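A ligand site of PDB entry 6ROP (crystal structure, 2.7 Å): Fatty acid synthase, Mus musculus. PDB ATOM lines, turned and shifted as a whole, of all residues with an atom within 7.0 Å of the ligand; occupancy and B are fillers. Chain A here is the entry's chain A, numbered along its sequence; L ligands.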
ATOM      1  N   VAL A 111     -23.518   3.911 -13.064  1.00  0.00           N
ATOM      2  CA  VAL A 111     -22.266   4.373 -12.411  1.00  0.00           C
ATOM      3  C   VAL A 111     -21.963   5.756 -12.976  1.00  0.00           C
ATOM      4  O   VAL A 111     -22.067   5.900 -14.178  1.00  0.00           O
ATOM      5  CB  VAL A 111     -21.100   3.407 -12.657  1.00  0.00           C
ATOM      6  CG1 VAL A 111     -20.884   3.123 -14.141  1.00  0.00           C
ATOM      7  CG2 VAL A 111     -19.820   3.922 -12.046  1.00  0.00           C
ATOM      8  N   SER A 112     -21.603   6.705 -12.127  1.00  0.00           N
ATOM      9  CA  SER A 112     -21.410   8.132 -12.502  1.00  0.00           C
ATOM     10  C   SER A 112     -20.002   8.603 -12.200  1.00  0.00           C
ATOM     11  O   SER A 112     -19.717   9.771 -12.481  1.00  0.00           O
ATOM     12  CB  SER A 112     -22.424   8.999 -11.814  1.00  0.00           C
ATOM     13  OG  SER A 112     -23.732   8.703 -12.288  1.00  0.00           O
ATOM     14  N   GLY A 113     -19.115   7.763 -11.676  1.00  0.00           N
ATOM     15  CA  GLY A 113     -17.744   8.226 -11.401  1.00  0.00           C
ATOM     16  C   GLY A 113     -16.789   7.092 -11.085  1.00  0.00           C
ATOM     17  O   GLY A 113     -17.210   6.133 -10.431  1.00  0.00           O
ATOM     18  N   GLU A 115     -13.638   7.920  -9.392  1.00  0.00           N
ATOM     19  CA  GLU A 115     -12.615   8.566  -8.546  1.00  0.00           C
ATOM     20  C   GLU A 115     -11.380   7.656  -8.512  1.00  0.00           C
ATOM     21  O   GLU A 115     -10.293   8.155  -8.746  1.00  0.00           O
ATOM     22  CB  GLU A 115     -13.246   8.892  -7.185  1.00  0.00           C
ATOM     23  CG  GLU A 115     -14.214  10.082  -7.214  1.00  0.00           C
ATOM     24  CD  GLU A 115     -15.118  10.290  -5.997  1.00  0.00           C
ATOM     25  OE1 GLU A 115     -15.243   9.355  -5.162  1.00  0.00           O
ATOM     26  OE2 GLU A 115     -15.712  11.378  -5.904  1.00  0.00           O
ATOM     27  N   ARG A 137     -14.984   2.634 -16.925  1.00  0.00           N
ATOM     28  CA  ARG A 137     -16.401   2.405 -16.558  1.00  0.00           C
ATOM     29  C   ARG A 137     -16.998   1.185 -17.274  1.00  0.00           C
ATOM     30  O   ARG A 137     -17.787   0.479 -16.636  1.00  0.00           O
ATOM     31  CB  ARG A 137     -17.273   3.610 -16.875  1.00  0.00           C
ATOM     32  CG  ARG A 137     -16.987   4.807 -15.986  1.00  0.00           C
ATOM     33  CD  ARG A 137     -18.242   5.641 -15.958  1.00  0.00           C
ATOM     34  NE  ARG A 137     -17.918   6.976 -15.498  1.00  0.00           N
ATOM     35  CZ  ARG A 137     -18.750   7.988 -15.571  1.00  0.00           C
ATOM     36  NH1 ARG A 137     -19.962   7.813 -16.061  1.00  0.00           N
ATOM     37  NH2 ARG A 137     -18.363   9.174 -15.134  1.00  0.00           N
ATOM     38  N   ASP A 158     -24.607   6.258 -17.532  1.00  0.00           N
ATOM     39  CA  ASP A 158     -24.666   7.481 -16.695  1.00  0.00           C
ATOM     40  C   ASP A 158     -25.829   8.341 -17.199  1.00  0.00           C
ATOM     41  O   ASP A 158     -25.842   8.764 -18.374  1.00  0.00           O
ATOM     42  CB  ASP A 158     -23.340   8.229 -16.687  1.00  0.00           C
ATOM     43  CG  ASP A 158     -23.182   9.181 -15.513  1.00  0.00           C
ATOM     44  OD1 ASP A 158     -24.187   9.360 -14.761  1.00  0.00           O
ATOM     45  OD2 ASP A 158     -22.075   9.746 -15.352  1.00  0.00           O
ATOM     46  N   THR A 159     -26.812   8.519 -16.322  1.00  0.00           N
ATOM     47  CA  THR A 159     -27.858   9.552 -16.387  1.00  0.00           C
ATOM     48  C   THR A 159     -27.859  10.225 -15.008  1.00  0.00           C
ATOM     49  O   THR A 159     -28.927  10.610 -14.543  1.00  0.00           O
ATOM     50  CB  THR A 159     -29.205   8.927 -16.774  1.00  0.00           C
ATOM     51  OG1 THR A 159     -29.662   8.130 -15.675  1.00  0.00           O
ATOM     52  CG2 THR A 159     -29.105   8.091 -18.029  1.00  0.00           C
ATOM     53  N   ALA A 160     -26.687  10.330 -14.399  1.00  0.00           N
ATOM     54  CA  ALA A 160     -26.517  10.853 -13.027  1.00  0.00           C
ATOM     55  C   ALA A 160     -27.396  10.020 -12.079  1.00  0.00           C
ATOM     56  O   ALA A 160     -27.322   8.783 -12.163  1.00  0.00           O
ATOM     57  CB  ALA A 160     -26.829  12.318 -13.011  1.00  0.00           C
ATOM     58  N   CYS A 161     -28.240  10.646 -11.273  1.00  0.00           N
ATOM     59  CA  CYS A 161     -28.918  10.024 -10.102  1.00  0.00           C
ATOM     60  C   CYS A 161     -29.914   8.929 -10.515  1.00  0.00           C
ATOM     61  O   CYS A 161     -30.131   7.979  -9.737  1.00  0.00           O
ATOM     62  CB  CYS A 161     -29.561  11.141  -9.294  1.00  0.00           C
ATOM     63  SG  CYS A 161     -28.295  12.081  -8.486  1.00  0.00           S
ATOM     64  N   SER A 162     -30.474   9.025 -11.722  1.00  0.00           N
ATOM     65  CA  SER A 162     -31.465   8.063 -12.285  1.00  0.00           C
ATOM     66  C   SER A 162     -30.770   6.840 -12.912  1.00  0.00           C
ATOM     67  O   SER A 162     -31.497   5.917 -13.349  1.00  0.00           O
ATOM     68  CB  SER A 162     -32.363   8.743 -13.272  1.00  0.00           C
ATOM     69  OG  SER A 162     -31.646   9.279 -14.383  1.00  0.00           O
ATOM     70  N   ASN A 189     -21.669   3.749  -6.154  1.00  0.00           N
ATOM     71  CA  ASN A 189     -21.273   5.134  -5.820  1.00  0.00           C
ATOM     72  C   ASN A 189     -20.338   5.107  -4.609  1.00  0.00           C
ATOM     73  O   ASN A 189     -20.685   4.439  -3.614  1.00  0.00           O
ATOM     74  CB  ASN A 189     -22.485   6.033  -5.608  1.00  0.00           C
ATOM     75  CG  ASN A 189     -22.102   7.481  -5.769  1.00  0.00           C
ATOM     76  OD1 ASN A 189     -21.441   7.833  -6.732  1.00  0.00           O
ATOM     77  ND2 ASN A 189     -22.470   8.312  -4.810  1.00  0.00           N
ATOM     78  N   LEU A 190     -19.196   5.785  -4.718  1.00  0.00           N
ATOM     79  CA  LEU A 190     -18.245   5.985  -3.586  1.00  0.00           C
ATOM     80  C   LEU A 190     -17.873   7.471  -3.481  1.00  0.00           C
ATOM     81  O   LEU A 190     -17.956   8.202  -4.498  1.00  0.00           O
ATOM     82  CB  LEU A 190     -16.975   5.155  -3.774  1.00  0.00           C
ATOM     83  CG  LEU A 190     -17.174   3.655  -3.954  1.00  0.00           C
ATOM     84  CD1 LEU A 190     -15.811   3.004  -4.132  1.00  0.00           C
ATOM     85  CD2 LEU A 190     -17.923   3.014  -2.786  1.00  0.00           C
ATOM     86  N   THR A 196     -15.015  16.563  -5.410  1.00  0.00           N
ATOM     87  CA  THR A 196     -16.337  16.255  -5.989  1.00  0.00           C
ATOM     88  C   THR A 196     -17.449  16.813  -5.089  1.00  0.00           C
ATOM     89  O   THR A 196     -18.444  17.313  -5.608  1.00  0.00           O
ATOM     90  CB  THR A 196     -16.479  14.749  -6.212  1.00  0.00           C
ATOM     91  OG1 THR A 196     -15.350  14.353  -7.004  1.00  0.00           O
ATOM     92  CG2 THR A 196     -17.777  14.400  -6.882  1.00  0.00           C
ATOM     93  N   GLN A 199     -17.542  20.804  -5.502  1.00  0.00           N
ATOM     94  CA  GLN A 199     -18.383  21.051  -6.709  1.00  0.00           C
ATOM     95  C   GLN A 199     -19.857  21.079  -6.277  1.00  0.00           C
ATOM     96  O   GLN A 199     -20.489  22.150  -6.457  1.00  0.00           O
ATOM     97  CB  GLN A 199     -18.140  20.011  -7.797  1.00  0.00           C
ATOM     98  CG  GLN A 199     -16.916  20.264  -8.680  1.00  0.00           C
ATOM     99  CD  GLN A 199     -16.612  19.097  -9.587  1.00  0.00           C
ATOM    100  OE1 GLN A 199     -16.194  18.033  -9.135  1.00  0.00           O
ATOM    101  NE2 GLN A 199     -16.834  19.280 -10.875  1.00  0.00           N
ATOM    102  N   PHE A 200     -20.377  19.987  -5.711  1.00  0.00           N
ATOM    103  CA  PHE A 200     -21.841  19.906  -5.420  1.00  0.00           C
ATOM    104  C   PHE A 200     -22.244  20.974  -4.405  1.00  0.00           C
ATOM    105  O   PHE A 200     -23.336  21.572  -4.545  1.00  0.00           O
ATOM    106  CB  PHE A 200     -22.265  18.520  -4.925  1.00  0.00           C
ATOM    107  CG  PHE A 200     -22.296  17.479  -6.005  1.00  0.00           C
ATOM    108  CD1 PHE A 200     -23.000  17.714  -7.182  1.00  0.00           C
ATOM    109  CD2 PHE A 200     -21.631  16.279  -5.851  1.00  0.00           C
ATOM    110  CE1 PHE A 200     -23.011  16.777  -8.189  1.00  0.00           C
ATOM    111  CE2 PHE A 200     -21.662  15.333  -6.862  1.00  0.00           C
ATOM    112  CZ  PHE A 200     -22.347  15.586  -8.025  1.00  0.00           C
ATOM    113  N   MET A 205     -26.221  22.196  -3.887  1.00  0.00           N
ATOM    114  CA  MET A 205     -27.022  20.939  -3.948  1.00  0.00           C
ATOM    115  C   MET A 205     -26.966  20.152  -2.636  1.00  0.00           C
ATOM    116  O   MET A 205     -27.791  19.230  -2.499  1.00  0.00           O
ATOM    117  CB  MET A 205     -26.506  20.052  -5.082  1.00  0.00           C
ATOM    118  CG  MET A 205     -26.362  20.787  -6.388  1.00  0.00           C
ATOM    119  SD  MET A 205     -25.734  19.722  -7.681  1.00  0.00           S
ATOM    120  CE  MET A 205     -27.266  18.958  -8.190  1.00  0.00           C
ATOM    121  N   TYR A 222     -29.130  17.762  -0.225  1.00  0.00           N
ATOM    122  CA  TYR A 222     -29.012  16.304   0.034  1.00  0.00           C
ATOM    123  C   TYR A 222     -27.709  15.983   0.800  1.00  0.00           C
ATOM    124  O   TYR A 222     -26.793  16.837   0.986  1.00  0.00           O
ATOM    125  CB  TYR A 222     -29.341  15.523  -1.253  1.00  0.00           C
ATOM    126  CG  TYR A 222     -28.284  15.463  -2.332  1.00  0.00           C
ATOM    127  CD1 TYR A 222     -27.223  14.597  -2.220  1.00  0.00           C
ATOM    128  CD2 TYR A 222     -28.395  16.196  -3.495  1.00  0.00           C
ATOM    129  CE1 TYR A 222     -26.262  14.488  -3.206  1.00  0.00           C
ATOM    130  CE2 TYR A 222     -27.441  16.110  -4.501  1.00  0.00           C
ATOM    131  CZ  TYR A 222     -26.374  15.231  -4.359  1.00  0.00           C
ATOM    132  OH  TYR A 222     -25.406  15.101  -5.325  1.00  0.00           O
ATOM    133  N   ARG A 224     -24.696  13.376   0.540  1.00  0.00           N
ATOM    134  CA  ARG A 224     -24.013  12.419  -0.371  1.00  0.00           C
ATOM    135  C   ARG A 224     -23.757  11.109   0.380  1.00  0.00           C
ATOM    136  O   ARG A 224     -23.435  11.165   1.573  1.00  0.00           O
ATOM    137  CB  ARG A 224     -22.686  12.944  -0.910  1.00  0.00           C
ATOM    138  CG  ARG A 224     -22.807  14.246  -1.690  1.00  0.00           C
ATOM    139  CD  ARG A 224     -21.498  14.494  -2.398  1.00  0.00           C
ATOM    140  NE  ARG A 224     -21.407  13.589  -3.539  1.00  0.00           N
ATOM    141  CZ  ARG A 224     -20.286  13.162  -4.091  1.00  0.00           C
ATOM    142  NH1 ARG A 224     -19.106  13.550  -3.629  1.00  0.00           N
ATOM    143  NH2 ARG A 224     -20.351  12.358  -5.125  1.00  0.00           N
ATOM    144  N   HIS A 293     -38.327   9.972  -5.110  1.00  0.00           N
ATOM    145  CA  HIS A 293     -36.897  10.338  -5.220  1.00  0.00           C
ATOM    146  C   HIS A 293     -36.515  10.985  -3.896  1.00  0.00           C
ATOM    147  O   HIS A 293     -35.555  10.538  -3.286  1.00  0.00           O
ATOM    148  CB  HIS A 293     -36.683  11.236  -6.440  1.00  0.00           C
ATOM    149  CG  HIS A 293     -35.270  11.566  -6.708  1.00  0.00           C
ATOM    150  ND1 HIS A 293     -34.333  10.609  -7.040  1.00  0.00           N
ATOM    151  CD2 HIS A 293     -34.614  12.758  -6.696  1.00  0.00           C
ATOM    152  CE1 HIS A 293     -33.164  11.191  -7.203  1.00  0.00           C
ATOM    153  NE2 HIS A 293     -33.298  12.498  -6.990  1.00  0.00           N
ATOM    154  N   HIS A 331     -28.348  10.174  -0.136  1.00  0.00           N
ATOM    155  CA  HIS A 331     -28.528  10.070  -1.595  1.00  0.00           C
ATOM    156  C   HIS A 331     -27.240   9.424  -2.069  1.00  0.00           C
ATOM    157  O   HIS A 331     -26.168   9.976  -1.874  1.00  0.00           O
ATOM    158  CB  HIS A 331     -28.815  11.483  -2.138  1.00  0.00           C
ATOM    159  CG  HIS A 331     -29.219  11.537  -3.568  1.00  0.00           C
ATOM    160  ND1 HIS A 331     -29.424  10.409  -4.327  1.00  0.00           N
ATOM    161  CD2 HIS A 331     -29.472  12.581  -4.371  1.00  0.00           C
ATOM    162  CE1 HIS A 331     -29.786  10.766  -5.542  1.00  0.00           C
ATOM    163  NE2 HIS A 331     -29.838  12.095  -5.588  1.00  0.00           N
ATOM    164  N   GLU A 333     -26.706   8.923  -5.106  1.00  0.00           N
ATOM    165  CA  GLU A 333     -26.536   9.491  -6.463  1.00  0.00           C
ATOM    166  C   GLU A 333     -27.019   8.423  -7.443  1.00  0.00           C
ATOM    167  O   GLU A 333     -28.176   8.026  -7.334  1.00  0.00           O
ATOM    168  CB  GLU A 333     -25.147  10.137  -6.545  1.00  0.00           C
ATOM    169  CG  GLU A 333     -25.084  11.374  -5.647  1.00  0.00           C
ATOM    170  CD  GLU A 333     -23.731  11.972  -5.302  1.00  0.00           C
ATOM    171  OE1 GLU A 333     -22.730  11.268  -5.429  1.00  0.00           O
ATOM    172  OE2 GLU A 333     -23.694  13.151  -4.890  1.00  0.00           O
ATOM    173  N   PRO A 334     -26.198   7.868  -8.358  1.00  0.00           N
ATOM    174  CA  PRO A 334     -26.710   6.965  -9.390  1.00  0.00           C
ATOM    175  C   PRO A 334     -27.263   5.624  -8.840  1.00  0.00           C
ATOM    176  O   PRO A 334     -28.199   5.052  -9.392  1.00  0.00           O
ATOM    177  CB  PRO A 334     -25.477   6.715 -10.254  1.00  0.00           C
ATOM    178  CG  PRO A 334     -24.316   6.860  -9.308  1.00  0.00           C
ATOM    179  CD  PRO A 334     -24.736   7.975  -8.374  1.00  0.00           C
ATOM    180  N   PHE A 393     -34.733  10.426 -10.481  1.00  0.00           N
ATOM    181  CA  PHE A 393     -34.496  11.595 -11.359  1.00  0.00           C
ATOM    182  C   PHE A 393     -33.013  11.976 -11.287  1.00  0.00           C
ATOM    183  O   PHE A 393     -32.477  12.019 -10.173  1.00  0.00           O
ATOM    184  CB  PHE A 393     -35.346  12.774 -10.913  1.00  0.00           C
ATOM    185  CG  PHE A 393     -36.799  12.440 -10.713  1.00  0.00           C
ATOM    186  CD1 PHE A 393     -37.439  11.517 -11.512  1.00  0.00           C
ATOM    187  CD2 PHE A 393     -37.514  13.036  -9.697  1.00  0.00           C
ATOM    188  CE1 PHE A 393     -38.779  11.193 -11.324  1.00  0.00           C
ATOM    189  CE2 PHE A 393     -38.856  12.702  -9.499  1.00  0.00           C
ATOM    190  CZ  PHE A 393     -39.493  11.791 -10.317  1.00  0.00           C
ATOM    191  N   GLY A 394     -32.403  12.255 -12.447  1.00  0.00           N
ATOM    192  CA  GLY A 394     -31.067  12.875 -12.581  1.00  0.00           C
ATOM    193  C   GLY A 394     -31.133  14.398 -12.775  1.00  0.00           C
ATOM    194  O   GLY A 394     -32.189  14.931 -13.220  1.00  0.00           O
ATOM    195  N   PHE A 395     -30.027  15.070 -12.462  1.00  0.00           N
ATOM    196  CA  PHE A 395     -29.926  16.559 -12.501  1.00  0.00           C
ATOM    197  C   PHE A 395     -29.915  17.026 -13.953  1.00  0.00           C
ATOM    198  O   PHE A 395     -30.258  18.189 -14.160  1.00  0.00           O
ATOM    199  CB  PHE A 395     -28.818  17.056 -11.564  1.00  0.00           C
ATOM    200  CG  PHE A 395     -27.388  17.003 -12.045  1.00  0.00           C
ATOM    201  CD1 PHE A 395     -26.898  15.931 -12.772  1.00  0.00           C
ATOM    202  CD2 PHE A 395     -26.503  18.015 -11.707  1.00  0.00           C
ATOM    203  CE1 PHE A 395     -25.577  15.903 -13.197  1.00  0.00           C
ATOM    204  CE2 PHE A 395     -25.182  17.998 -12.132  1.00  0.00           C
ATOM    205  CZ  PHE A 395     -24.720  16.937 -12.872  1.00  0.00           C
ATOM    206  N   GLY A 396     -29.646  16.146 -14.931  1.00  0.00           N
ATOM    207  CA  GLY A 396     -29.651  16.471 -16.367  1.00  0.00           C
ATOM    208  C   GLY A 396     -31.035  16.407 -16.975  1.00  0.00           C
ATOM    209  O   GLY A 396     -31.222  16.850 -18.135  1.00  0.00           O
HETATM  210  C1  LIG L   1     -27.659  13.400  -9.248  1.00  0.00           C
HETATM  211  C2  LIG L   1     -26.364  14.048  -8.786  1.00  0.00           C
HETATM  212  C3  LIG L   1     -25.223  14.093  -9.803  1.00  0.00           C
HETATM  213  C4  LIG L   1     -24.583  12.741 -10.093  1.00  0.00           C
HETATM  214  C5  LIG L   1     -23.071  12.735 -10.314  1.00  0.00           C
HETATM  215  C6  LIG L   1     -22.296  11.930  -9.266  1.00  0.00           C
HETATM  216  C7  LIG L   1     -20.876  11.541  -9.585  1.00  0.00           C
HETATM  217  C8  LIG L   1     -20.015  12.591 -10.264  1.00  0.00           C
HETATM  218  O1  LIG L   1     -28.248  13.857 -10.226  1.00  0.00           O
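O of Ser 112 touches C7 of the ligand, 3.6 Å away. Ala 160 touches the ligand (CB to O1, 3.5 Å). CZ of Phe 200 touches C3 of the ligand, 3.7 Å away. Tyr 222 touches the ligand (OH to C2, 3.7 Å). Glu 333 touches the ligand (OE1 to C6, 3.9 Å). Gly 394 touches the ligand (CA to O1, 3.8 Å). Hydrophobic or aromatic side chains within 4 Å of the ligand: Ala 160, Phe 200 and Phe 395.
N of Glu 333 lies close to ND1 of His 331, 3.2 Å away. OE1 of Glu 333 is in hydrogen-bond range of ND2 of Asn 189 (3.0 Å). The backbone carbonyl oxygen of Phe 200 sits at hydrogen-bond distance from the backbone NH of Met 205, at 3.0 Å. N of Ala 160 sits at hydrogen-bond distance from OD1 of Asp 158, 2.7 Å away. The side-chain hydroxyl (OG) of Ser 112 lies within hydrogen-bond range of the side-chain carboxylate (OD1) of Asp 158 (2.6 Å). O of Ser 112 sits at hydrogen-bond distance from NH2 of Arg 137, at 3.0 Å. The side-chain carboxylate of Glu 333 is in salt-bridge range of the guanidinium group of Arg 224, at 2.6 Å. The backbone NH (N) of Tyr 222 sits at hydrogen-bond distance from the backbone carbonyl oxygen (O) of Met 205 (3.0 Å).
The backbone NH (N) of Cys 161 sits close to an oxygen (O1) of the ligand (3.4 Å). A carbon (C1) of the ligand is covalently linked to the side-chain sulfur of Cys 161, at 1.7 Å. The backbone NH (N) of Phe 395 lies within hydrogen-bond range of an oxygen (O1) of the ligand (3.1 Å).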
